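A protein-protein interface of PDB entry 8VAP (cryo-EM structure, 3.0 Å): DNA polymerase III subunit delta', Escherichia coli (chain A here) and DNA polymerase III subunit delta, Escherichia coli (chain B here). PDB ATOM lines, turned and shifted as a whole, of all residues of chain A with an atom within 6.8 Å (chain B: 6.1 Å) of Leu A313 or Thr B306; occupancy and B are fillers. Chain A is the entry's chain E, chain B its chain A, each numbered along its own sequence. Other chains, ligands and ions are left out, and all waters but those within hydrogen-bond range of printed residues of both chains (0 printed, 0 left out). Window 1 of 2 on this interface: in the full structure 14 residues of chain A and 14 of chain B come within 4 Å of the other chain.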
ATOM      1  N   LEU A 236      -7.104 -20.468  19.353  1.00  0.00           N
ATOM      2  CA  LEU A 236      -6.698 -20.943  18.033  1.00  0.00           C
ATOM      3  C   LEU A 236      -6.196 -22.381  18.082  1.00  0.00           C
ATOM      4  O   LEU A 236      -6.732 -23.266  17.404  1.00  0.00           O
ATOM      5  CB  LEU A 236      -5.621 -20.019  17.463  1.00  0.00           C
ATOM      6  CG  LEU A 236      -5.224 -20.217  16.000  1.00  0.00           C
ATOM      7  CD1 LEU A 236      -6.443 -20.431  15.130  1.00  0.00           C
ATOM      8  CD2 LEU A 236      -4.413 -19.033  15.505  1.00  0.00           C
ATOM      9  N   ASN A 240      -7.898 -25.602  15.849  1.00  0.00           N
ATOM     10  CA  ASN A 240      -7.344 -25.862  14.522  1.00  0.00           C
ATOM     11  C   ASN A 240      -6.571 -27.183  14.507  1.00  0.00           C
ATOM     12  O   ASN A 240      -5.355 -27.228  14.322  1.00  0.00           O
ATOM     13  CB  ASN A 240      -6.467 -24.689  14.086  1.00  0.00           C
ATOM     14  CG  ASN A 240      -5.923 -24.853  12.683  1.00  0.00           C
ATOM     15  OD1 ASN A 240      -6.587 -25.401  11.806  1.00  0.00           O
ATOM     16  ND2 ASN A 240      -4.706 -24.372  12.463  1.00  0.00           N
ATOM     17  N   ILE A 299     -19.248 -19.623  10.450  1.00  0.00           N
ATOM     18  CA  ILE A 299     -17.900 -20.062  10.106  1.00  0.00           C
ATOM     19  C   ILE A 299     -17.826 -21.582  10.041  1.00  0.00           C
ATOM     20  O   ILE A 299     -17.139 -22.144   9.182  1.00  0.00           O
ATOM     21  CB  ILE A 299     -16.874 -19.479  11.093  1.00  0.00           C
ATOM     22  CG1 ILE A 299     -16.822 -17.958  10.950  1.00  0.00           C
ATOM     23  CG2 ILE A 299     -15.499 -20.079  10.862  1.00  0.00           C
ATOM     24  CD1 ILE A 299     -16.513 -17.497   9.542  1.00  0.00           C
ATOM     25  N   GLN A 302     -19.262 -22.490   6.726  1.00  0.00           N
ATOM     26  CA  GLN A 302     -18.319 -22.209   5.648  1.00  0.00           C
ATOM     27  C   GLN A 302     -17.202 -23.244   5.605  1.00  0.00           C
ATOM     28  O   GLN A 302     -16.761 -23.649   4.524  1.00  0.00           O
ATOM     29  CB  GLN A 302     -17.744 -20.804   5.806  1.00  0.00           C
ATOM     30  CG  GLN A 302     -18.656 -19.708   5.292  1.00  0.00           C
ATOM     31  CD  GLN A 302     -18.040 -18.332   5.415  1.00  0.00           C
ATOM     32  OE1 GLN A 302     -17.139 -18.114   6.226  1.00  0.00           O
ATOM     33  NE2 GLN A 302     -18.521 -17.393   4.610  1.00  0.00           N
ATOM     34  N   ILE A 309     -10.501 -24.943   1.657  1.00  0.00           N
ATOM     35  CA  ILE A 309     -10.355 -23.698   2.397  1.00  0.00           C
ATOM     36  C   ILE A 309      -9.318 -23.873   3.505  1.00  0.00           C
ATOM     37  O   ILE A 309      -9.048 -24.983   3.980  1.00  0.00           O
ATOM     38  CB  ILE A 309     -11.715 -23.257   2.965  1.00  0.00           C
ATOM     39  CG1 ILE A 309     -11.690 -21.783   3.369  1.00  0.00           C
ATOM     40  CG2 ILE A 309     -12.111 -24.128   4.147  1.00  0.00           C
ATOM     41  CD1 ILE A 309     -11.551 -20.840   2.205  1.00  0.00           C
ATOM     42  N   ASN A 310      -8.716 -22.756   3.914  1.00  0.00           N
ATOM     43  CA  ASN A 310      -7.740 -22.761   4.999  1.00  0.00           C
ATOM     44  C   ASN A 310      -8.477 -22.707   6.330  1.00  0.00           C
ATOM     45  O   ASN A 310      -9.149 -21.718   6.638  1.00  0.00           O
ATOM     46  CB  ASN A 310      -6.767 -21.594   4.878  1.00  0.00           C
ATOM     47  CG  ASN A 310      -5.416 -21.903   5.494  1.00  0.00           C
ATOM     48  OD1 ASN A 310      -5.005 -23.061   5.569  1.00  0.00           O
ATOM     49  ND2 ASN A 310      -4.713 -20.865   5.930  1.00  0.00           N
ATOM     50  N   ARG A 311      -8.345 -23.773   7.116  1.00  0.00           N
ATOM     51  CA  ARG A 311      -8.950 -23.799   8.440  1.00  0.00           C
ATOM     52  C   ARG A 311      -8.331 -22.748   9.351  1.00  0.00           C
ATOM     53  O   ARG A 311      -9.046 -22.046  10.078  1.00  0.00           O
ATOM     54  CB  ARG A 311      -8.794 -25.196   9.037  1.00  0.00           C
ATOM     55  CG  ARG A 311      -9.435 -25.392  10.388  1.00  0.00           C
ATOM     56  CD  ARG A 311      -9.298 -26.841  10.824  1.00  0.00           C
ATOM     57  NE  ARG A 311      -7.903 -27.257  10.904  1.00  0.00           N
ATOM     58  CZ  ARG A 311      -7.313 -28.062  10.032  1.00  0.00           C
ATOM     59  NH1 ARG A 311      -7.969 -28.558   8.996  1.00  0.00           N
ATOM     60  NH2 ARG A 311      -6.031 -28.374  10.201  1.00  0.00           N
ATOM     61  N   GLU A 312      -7.003 -22.617   9.316  1.00  0.00           N
ATOM     62  CA  GLU A 312      -6.317 -21.737  10.257  1.00  0.00           C
ATOM     63  C   GLU A 312      -6.706 -20.279  10.046  1.00  0.00           C
ATOM     64  O   GLU A 312      -6.977 -19.559  11.015  1.00  0.00           O
ATOM     65  CB  GLU A 312      -4.805 -21.912  10.128  1.00  0.00           C
ATOM     66  CG  GLU A 312      -4.006 -21.143  11.164  1.00  0.00           C
ATOM     67  CD  GLU A 312      -2.511 -21.351  11.019  1.00  0.00           C
ATOM     68  OE1 GLU A 312      -2.099 -22.098  10.108  1.00  0.00           O
ATOM     69  OE2 GLU A 312      -1.748 -20.764  11.815  1.00  0.00           O
ATOM     70  N   LEU A 313      -6.738 -19.823   8.791  1.00  0.00           N
ATOM     71  CA  LEU A 313      -7.102 -18.434   8.530  1.00  0.00           C
ATOM     72  C   LEU A 313      -8.536 -18.150   8.958  1.00  0.00           C
ATOM     73  O   LEU A 313      -8.816 -17.106   9.559  1.00  0.00           O
ATOM     74  CB  LEU A 313      -6.917 -18.102   7.050  1.00  0.00           C
ATOM     75  CG  LEU A 313      -7.402 -16.704   6.660  1.00  0.00           C
ATOM     76  CD1 LEU A 313      -6.723 -15.643   7.510  1.00  0.00           C
ATOM     77  CD2 LEU A 313      -7.171 -16.429   5.193  1.00  0.00           C
ATOM     78  N   LEU A 314      -9.459 -19.066   8.654  1.00  0.00           N
ATOM     79  CA  LEU A 314     -10.851 -18.854   9.031  1.00  0.00           C
ATOM     80  C   LEU A 314     -11.011 -18.796  10.543  1.00  0.00           C
ATOM     81  O   LEU A 314     -11.728 -17.933  11.063  1.00  0.00           O
ATOM     82  CB  LEU A 314     -11.735 -19.952   8.444  1.00  0.00           C
ATOM     83  CG  LEU A 314     -12.099 -19.829   6.966  1.00  0.00           C
ATOM     84  CD1 LEU A 314     -12.984 -20.984   6.550  1.00  0.00           C
ATOM     85  CD2 LEU A 314     -12.794 -18.512   6.699  1.00  0.00           C
ATOM     86  N   ILE A 315     -10.351 -19.699  11.269  1.00  0.00           N
ATOM     87  CA  ILE A 315     -10.485 -19.697  12.722  1.00  0.00           C
ATOM     88  C   ILE A 315      -9.848 -18.448  13.319  1.00  0.00           C
ATOM     89  O   ILE A 315     -10.380 -17.858  14.269  1.00  0.00           O
ATOM     90  CB  ILE A 315      -9.893 -20.986  13.319  1.00  0.00           C
ATOM     91  CG1 ILE A 315     -10.633 -22.207  12.776  1.00  0.00           C
ATOM     92  CG2 ILE A 315      -9.996 -20.962  14.828  1.00  0.00           C
ATOM     93  CD1 ILE A 315     -10.266 -23.499  13.467  1.00  0.00           C
ATOM     94  N   THR A 316      -8.707 -18.018  12.774  1.00  0.00           N
ATOM     95  CA  THR A 316      -8.075 -16.796  13.262  1.00  0.00           C
ATOM     96  C   THR A 316      -8.968 -15.583  13.032  1.00  0.00           C
ATOM     97  O   THR A 316      -9.102 -14.723  13.912  1.00  0.00           O
ATOM     98  CB  THR A 316      -6.722 -16.600  12.579  1.00  0.00           C
ATOM     99  OG1 THR A 316      -5.873 -17.717  12.872  1.00  0.00           O
ATOM    100  CG2 THR A 316      -6.059 -15.327  13.067  1.00  0.00           C
ATOM    101  N   ASP A 317      -9.590 -15.499  11.854  1.00  0.00           N
ATOM    102  CA  ASP A 317     -10.509 -14.400  11.578  1.00  0.00           C
ATOM    103  C   ASP A 317     -11.718 -14.446  12.501  1.00  0.00           C
ATOM    104  O   ASP A 317     -12.188 -13.406  12.973  1.00  0.00           O
ATOM    105  CB  ASP A 317     -10.954 -14.448  10.122  1.00  0.00           C
ATOM    106  CG  ASP A 317     -11.449 -13.117   9.628  1.00  0.00           C
ATOM    107  OD1 ASP A 317     -12.465 -12.620  10.155  1.00  0.00           O
ATOM    108  OD2 ASP A 317     -10.813 -12.564   8.715  1.00  0.00           O
ATOM    109  N   LEU A 318     -12.244 -15.647  12.751  1.00  0.00           N
ATOM    110  CA  LEU A 318     -13.344 -15.808  13.695  1.00  0.00           C
ATOM    111  C   LEU A 318     -12.972 -15.278  15.072  1.00  0.00           C
ATOM    112  O   LEU A 318     -13.744 -14.536  15.694  1.00  0.00           O
ATOM    113  CB  LEU A 318     -13.730 -17.286  13.773  1.00  0.00           C
ATOM    114  CG  LEU A 318     -14.797 -17.747  14.762  1.00  0.00           C
ATOM    115  CD1 LEU A 318     -16.114 -17.057  14.498  1.00  0.00           C
ATOM    116  CD2 LEU A 318     -14.955 -19.255  14.684  1.00  0.00           C
ATOM    117  N   ARG A 321     -12.688 -11.482  15.063  1.00  0.00           N
ATOM    118  CA  ARG A 321     -14.014 -10.875  15.036  1.00  0.00           C
ATOM    119  C   ARG A 321     -14.689 -10.961  16.399  1.00  0.00           C
ATOM    120  O   ARG A 321     -15.369 -10.018  16.817  1.00  0.00           O
ATOM    121  CB  ARG A 321     -14.875 -11.542  13.967  1.00  0.00           C
ATOM    122  CG  ARG A 321     -14.966 -10.754  12.675  1.00  0.00           C
ATOM    123  CD  ARG A 321     -16.315 -10.957  12.014  1.00  0.00           C
ATOM    124  NE  ARG A 321     -16.595 -12.369  11.790  1.00  0.00           N
ATOM    125  CZ  ARG A 321     -16.067 -13.093  10.814  1.00  0.00           C
ATOM    126  NH1 ARG A 321     -15.227 -12.565   9.938  1.00  0.00           N
ATOM    127  NH2 ARG A 321     -16.388 -14.379  10.713  1.00  0.00           N
ATOM    128  N   ARG B 248      -1.424 -17.528   0.097  1.00  0.00           N
ATOM    129  CA  ARG B 248      -0.871 -18.440   1.097  1.00  0.00           C
ATOM    130  C   ARG B 248       0.316 -17.820   1.823  1.00  0.00           C
ATOM    131  O   ARG B 248       0.395 -17.867   3.058  1.00  0.00           O
ATOM    132  CB  ARG B 248      -0.458 -19.766   0.454  1.00  0.00           C
ATOM    133  CG  ARG B 248      -1.564 -20.528  -0.258  1.00  0.00           C
ATOM    134  CD  ARG B 248      -2.658 -20.981   0.685  1.00  0.00           C
ATOM    135  NE  ARG B 248      -3.584 -19.900   0.996  1.00  0.00           N
ATOM    136  CZ  ARG B 248      -4.412 -19.908   2.027  1.00  0.00           C
ATOM    137  NH1 ARG B 248      -4.464 -20.934   2.856  1.00  0.00           N
ATOM    138  NH2 ARG B 248      -5.199 -18.858   2.238  1.00  0.00           N
ATOM    139  N   GLN B 251      -0.935 -15.122   4.054  1.00  0.00           N
ATOM    140  CA  GLN B 251      -1.558 -15.662   5.256  1.00  0.00           C
ATOM    141  C   GLN B 251      -0.514 -16.108   6.265  1.00  0.00           C
ATOM    142  O   GLN B 251      -0.619 -15.790   7.455  1.00  0.00           O
ATOM    143  CB  GLN B 251      -2.478 -16.827   4.887  1.00  0.00           C
ATOM    144  CG  GLN B 251      -2.934 -17.669   6.068  1.00  0.00           C
ATOM    145  CD  GLN B 251      -2.135 -18.946   6.219  1.00  0.00           C
ATOM    146  OE1 GLN B 251      -1.600 -19.474   5.245  1.00  0.00           O
ATOM    147  NE2 GLN B 251      -2.053 -19.451   7.442  1.00  0.00           N
ATOM    148  N   LEU B 255      -0.163 -14.101   9.759  1.00  0.00           N
ATOM    149  CA  LEU B 255      -0.450 -14.758  11.029  1.00  0.00           C
ATOM    150  C   LEU B 255       0.742 -14.664  11.971  1.00  0.00           C
ATOM    151  O   LEU B 255       0.578 -14.403  13.172  1.00  0.00           O
ATOM    152  CB  LEU B 255      -0.839 -16.216  10.794  1.00  0.00           C
ATOM    153  CG  LEU B 255      -2.188 -16.450  10.114  1.00  0.00           C
ATOM    154  CD1 LEU B 255      -2.654 -17.876  10.336  1.00  0.00           C
ATOM    155  CD2 LEU B 255      -3.229 -15.460  10.609  1.00  0.00           C
ATOM    156  N   ALA B 301      -6.843  -6.420   7.848  1.00  0.00           N
ATOM    157  CA  ALA B 301      -6.107  -7.205   6.862  1.00  0.00           C
ATOM    158  C   ALA B 301      -6.525  -8.667   6.899  1.00  0.00           C
ATOM    159  O   ALA B 301      -6.699  -9.295   5.849  1.00  0.00           O
ATOM    160  CB  ALA B 301      -4.606  -7.070   7.100  1.00  0.00           C
ATOM    161  N   VAL B 302      -6.688  -9.228   8.098  1.00  0.00           N
ATOM    162  CA  VAL B 302      -7.137 -10.612   8.209  1.00  0.00           C
ATOM    163  C   VAL B 302      -8.535 -10.763   7.625  1.00  0.00           C
ATOM    164  O   VAL B 302      -8.828 -11.740   6.926  1.00  0.00           O
ATOM    165  CB  VAL B 302      -7.075 -11.085   9.673  1.00  0.00           C
ATOM    166  CG1 VAL B 302      -7.735 -12.444   9.820  1.00  0.00           C
ATOM    167  CG2 VAL B 302      -5.637 -11.151  10.143  1.00  0.00           C
ATOM    168  N   GLN B 303      -9.419  -9.799   7.896  1.00  0.00           N
ATOM    169  CA  GLN B 303     -10.774  -9.856   7.350  1.00  0.00           C
ATOM    170  C   GLN B 303     -10.755  -9.838   5.828  1.00  0.00           C
ATOM    171  O   GLN B 303     -11.444 -10.632   5.173  1.00  0.00           O
ATOM    172  CB  GLN B 303     -11.605  -8.693   7.890  1.00  0.00           C
ATOM    173  CG  GLN B 303     -13.068  -8.743   7.489  1.00  0.00           C
ATOM    174  CD  GLN B 303     -13.838  -7.525   7.954  1.00  0.00           C
ATOM    175  OE1 GLN B 303     -13.550  -6.401   7.545  1.00  0.00           O
ATOM    176  NE2 GLN B 303     -14.825  -7.742   8.817  1.00  0.00           N
ATOM    177  N   LEU B 304      -9.967  -8.935   5.246  1.00  0.00           N
ATOM    178  CA  LEU B 304      -9.921  -8.824   3.793  1.00  0.00           C
ATOM    179  C   LEU B 304      -9.298 -10.065   3.167  1.00  0.00           C
ATOM    180  O   LEU B 304      -9.756 -10.539   2.119  1.00  0.00           O
ATOM    181  CB  LEU B 304      -9.156  -7.563   3.399  1.00  0.00           C
ATOM    182  CG  LEU B 304      -9.130  -7.204   1.918  1.00  0.00           C
ATOM    183  CD1 LEU B 304     -10.530  -7.255   1.348  1.00  0.00           C
ATOM    184  CD2 LEU B 304      -8.550  -5.817   1.752  1.00  0.00           C
ATOM    185  N   LEU B 305      -8.259 -10.614   3.800  1.00  0.00           N
ATOM    186  CA  LEU B 305      -7.646 -11.843   3.305  1.00  0.00           C
ATOM    187  C   LEU B 305      -8.627 -13.007   3.362  1.00  0.00           C
ATOM    188  O   LEU B 305      -8.686 -13.826   2.437  1.00  0.00           O
ATOM    189  CB  LEU B 305      -6.390 -12.151   4.119  1.00  0.00           C
ATOM    190  CG  LEU B 305      -5.653 -13.458   3.843  1.00  0.00           C
ATOM    191  CD1 LEU B 305      -5.009 -13.424   2.477  1.00  0.00           C
ATOM    192  CD2 LEU B 305      -4.616 -13.722   4.919  1.00  0.00           C
ATOM    193  N   THR B 306      -9.402 -13.098   4.445  1.00  0.00           N
ATOM    194  CA  THR B 306     -10.403 -14.150   4.559  1.00  0.00           C
ATOM    195  C   THR B 306     -11.471 -14.016   3.484  1.00  0.00           C
ATOM    196  O   THR B 306     -11.870 -15.011   2.867  1.00  0.00           O
ATOM    197  CB  THR B 306     -11.034 -14.114   5.949  1.00  0.00           C
ATOM    198  OG1 THR B 306     -10.041 -14.421   6.936  1.00  0.00           O
ATOM    199  CG2 THR B 306     -12.171 -15.112   6.049  1.00  0.00           C
ATOM    200  N   ARG B 307     -11.944 -12.791   3.241  1.00  0.00           N
ATOM    201  CA  ARG B 307     -12.932 -12.585   2.187  1.00  0.00           C
ATOM    202  C   ARG B 307     -12.368 -12.963   0.825  1.00  0.00           C
ATOM    203  O   ARG B 307     -13.055 -13.589   0.009  1.00  0.00           O
ATOM    204  CB  ARG B 307     -13.408 -11.132   2.182  1.00  0.00           C
ATOM    205  CG  ARG B 307     -14.444 -10.807   3.241  1.00  0.00           C
ATOM    206  CD  ARG B 307     -14.709  -9.312   3.302  1.00  0.00           C
ATOM    207  NE  ARG B 307     -15.706  -8.969   4.309  1.00  0.00           N
ATOM    208  CZ  ARG B 307     -15.849  -7.763   4.840  1.00  0.00           C
ATOM    209  NH1 ARG B 307     -15.068  -6.754   4.486  1.00  0.00           N
ATOM    210  NH2 ARG B 307     -16.801  -7.562   5.747  1.00  0.00           N
ATOM    211  N   THR B 308     -11.111 -12.594   0.562  1.00  0.00           N
ATOM    212  CA  THR B 308     -10.491 -12.929  -0.714  1.00  0.00           C
ATOM    213  C   THR B 308     -10.363 -14.438  -0.894  1.00  0.00           C
ATOM    214  O   THR B 308     -10.662 -14.970  -1.971  1.00  0.00           O
ATOM    215  CB  THR B 308      -9.122 -12.258  -0.817  1.00  0.00           C
ATOM    216  OG1 THR B 308      -9.228 -10.891  -0.405  1.00  0.00           O
ATOM    217  CG2 THR B 308      -8.616 -12.306  -2.242  1.00  0.00           C
ATOM    218  N   GLU B 309      -9.922 -15.147   0.149  1.00  0.00           N
ATOM    219  CA  GLU B 309      -9.798 -16.596   0.030  1.00  0.00           C
ATOM    220  C   GLU B 309     -11.159 -17.254  -0.140  1.00  0.00           C
ATOM    221  O   GLU B 309     -11.292 -18.226  -0.889  1.00  0.00           O
ATOM    222  CB  GLU B 309      -9.081 -17.198   1.235  1.00  0.00           C
ATOM    223  CG  GLU B 309      -8.899 -18.701   1.067  1.00  0.00           C
ATOM    224  CD  GLU B 309      -8.248 -19.376   2.248  1.00  0.00           C
ATOM    225  OE1 GLU B 309      -7.968 -18.691   3.250  1.00  0.00           O
ATOM    226  OE2 GLU B 309      -8.014 -20.600   2.171  1.00  0.00           O
ATOM    227  N   LEU B 310     -12.179 -16.757   0.562  1.00  0.00           N
ATOM    228  CA  LEU B 310     -13.516 -17.312   0.385  1.00  0.00           C
ATOM    229  C   LEU B 310     -14.011 -17.097  -1.038  1.00  0.00           C
ATOM    230  O   LEU B 310     -14.611 -17.996  -1.635  1.00  0.00           O
ATOM    231  CB  LEU B 310     -14.486 -16.698   1.392  1.00  0.00           C
ATOM    232  CG  LEU B 310     -14.555 -17.399   2.749  1.00  0.00           C
ATOM    233  CD1 LEU B 310     -15.368 -16.578   3.734  1.00  0.00           C
ATOM    234  CD2 LEU B 310     -15.133 -18.797   2.600  1.00  0.00           C
ATOM    235  N   THR B 311     -13.758 -15.916  -1.601  1.00  0.00           N
ATOM    236  CA  THR B 311     -14.137 -15.668  -2.988  1.00  0.00           C
ATOM    237  C   THR B 311     -13.417 -16.624  -3.931  1.00  0.00           C
ATOM    238  O   THR B 311     -14.026 -17.166  -4.862  1.00  0.00           O
ATOM    239  CB  THR B 311     -13.836 -14.216  -3.361  1.00  0.00           C
ATOM    240  OG1 THR B 311     -14.765 -13.350  -2.698  1.00  0.00           O
ATOM    241  CG2 THR B 311     -13.950 -14.011  -4.863  1.00  0.00           C
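OG1 of Thr B306 is in hydrogen-bond range of OD2 of Asp A317 (2.7 Å).
The side-chain amide nitrogen of Asn A310 lies close to the side-chain amide nitrogen of Gln B251 (3.4 Å).
OD2 of Asp A317 sits close to O of Val B302, 2.8 Å away.
N of Asn A310 sits at hydrogen-bond distance from OE2 of Glu B309 (2.9 Å).
The guanidinium group (NH1) of Arg B248 sits close to the side-chain amide nitrogen (ND2) of Asn A310, at 3.1 Å.
The side-chain carboxylate (OD2) of Asp A317 sits close to the backbone NH (N) of Gln B303 (3.2 Å).
The side-chain amide oxygen (OE1) of Gln B303 lies within hydrogen-bond range of the guanidinium group (NH1) of Arg B307 (3.4 Å).
The side-chain amide oxygen (OE1) of Gln B251 sits close to the backbone carbonyl oxygen (O) of Arg B248, at 3.4 Å.
The backbone carbonyl oxygen (O) of Val B302 is in hydrogen-bond range of the side-chain hydroxyl (OG1) of Thr B306 (2.9 Å).
The side-chain hydroxyl (OG1) of Thr A316 is in hydrogen-bond range of the backbone carbonyl oxygen (O) of Glu A312.
NH2 of Arg B248 is in salt-bridge range of OE1 of Glu B309, 3.0 Å away.
The side-chain carboxylate (OD1) of Asp A317 lies within salt-bridge range of the guanidinium group (NH1) of Arg A321 (2.8 Å).
Among the printed residues, merely in contact across the chains: Leu A313 with Glu B309 (3.1 Å), Glu A312 with Leu B255 (3.4 Å), Gln A302 with Leu B310 (3.4 Å), Leu A313 with Thr B306 (3.5 Å), Leu A314 with Thr B306 (3.5 Å), Ile A309 with Glu B309 (3.5 Å), Leu A313 with Leu B305 (3.6 Å), Thr A316 with Leu B255 (3.8 Å) and Glu A312 with Gln B251 (3.8 Å).
Of chain B, only Leu B305 (3.6 Å), Thr B306 (3.5 Å) and Glu B309 (3.1 Å) come within 4 Å of Leu A313.
Of the printed residues of chain A, Val B302 touches Asp A317.
Of the printed residues of chain B, Glu A312 touches Gln B251 (3.8 Å) and Leu B255 (3.4 Å).
Printed residues of chain B within 4 Å of Ile A309: Glu B309.
Of the printed residues of chain A, Leu B255 touches Glu A312 and Thr A316.
The nearest residue of chain B that does not touch Leu A313 is Val B302 (4.1 Å).
The nearest printed residue of chain A that does not touch Leu B255 is Leu A313 (4.7 Å).
Of the 15 printed residues of chain A, 8 touch a printed residue of chain B.
Hydrophobic or aromatic side chains of chain A within 4 Å of the printed part of chain B: Ile A309, Leu A313 and Leu A314.
Of the 14 printed residues of chain B, 9 touch a printed residue of chain A.
Among the printed residues, 15 pairs touch across the chains.
Among the printed residues, no Asp or Glu carboxylate lies within 4 Å of a Lys or Arg side-chain nitrogen of the other chain.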
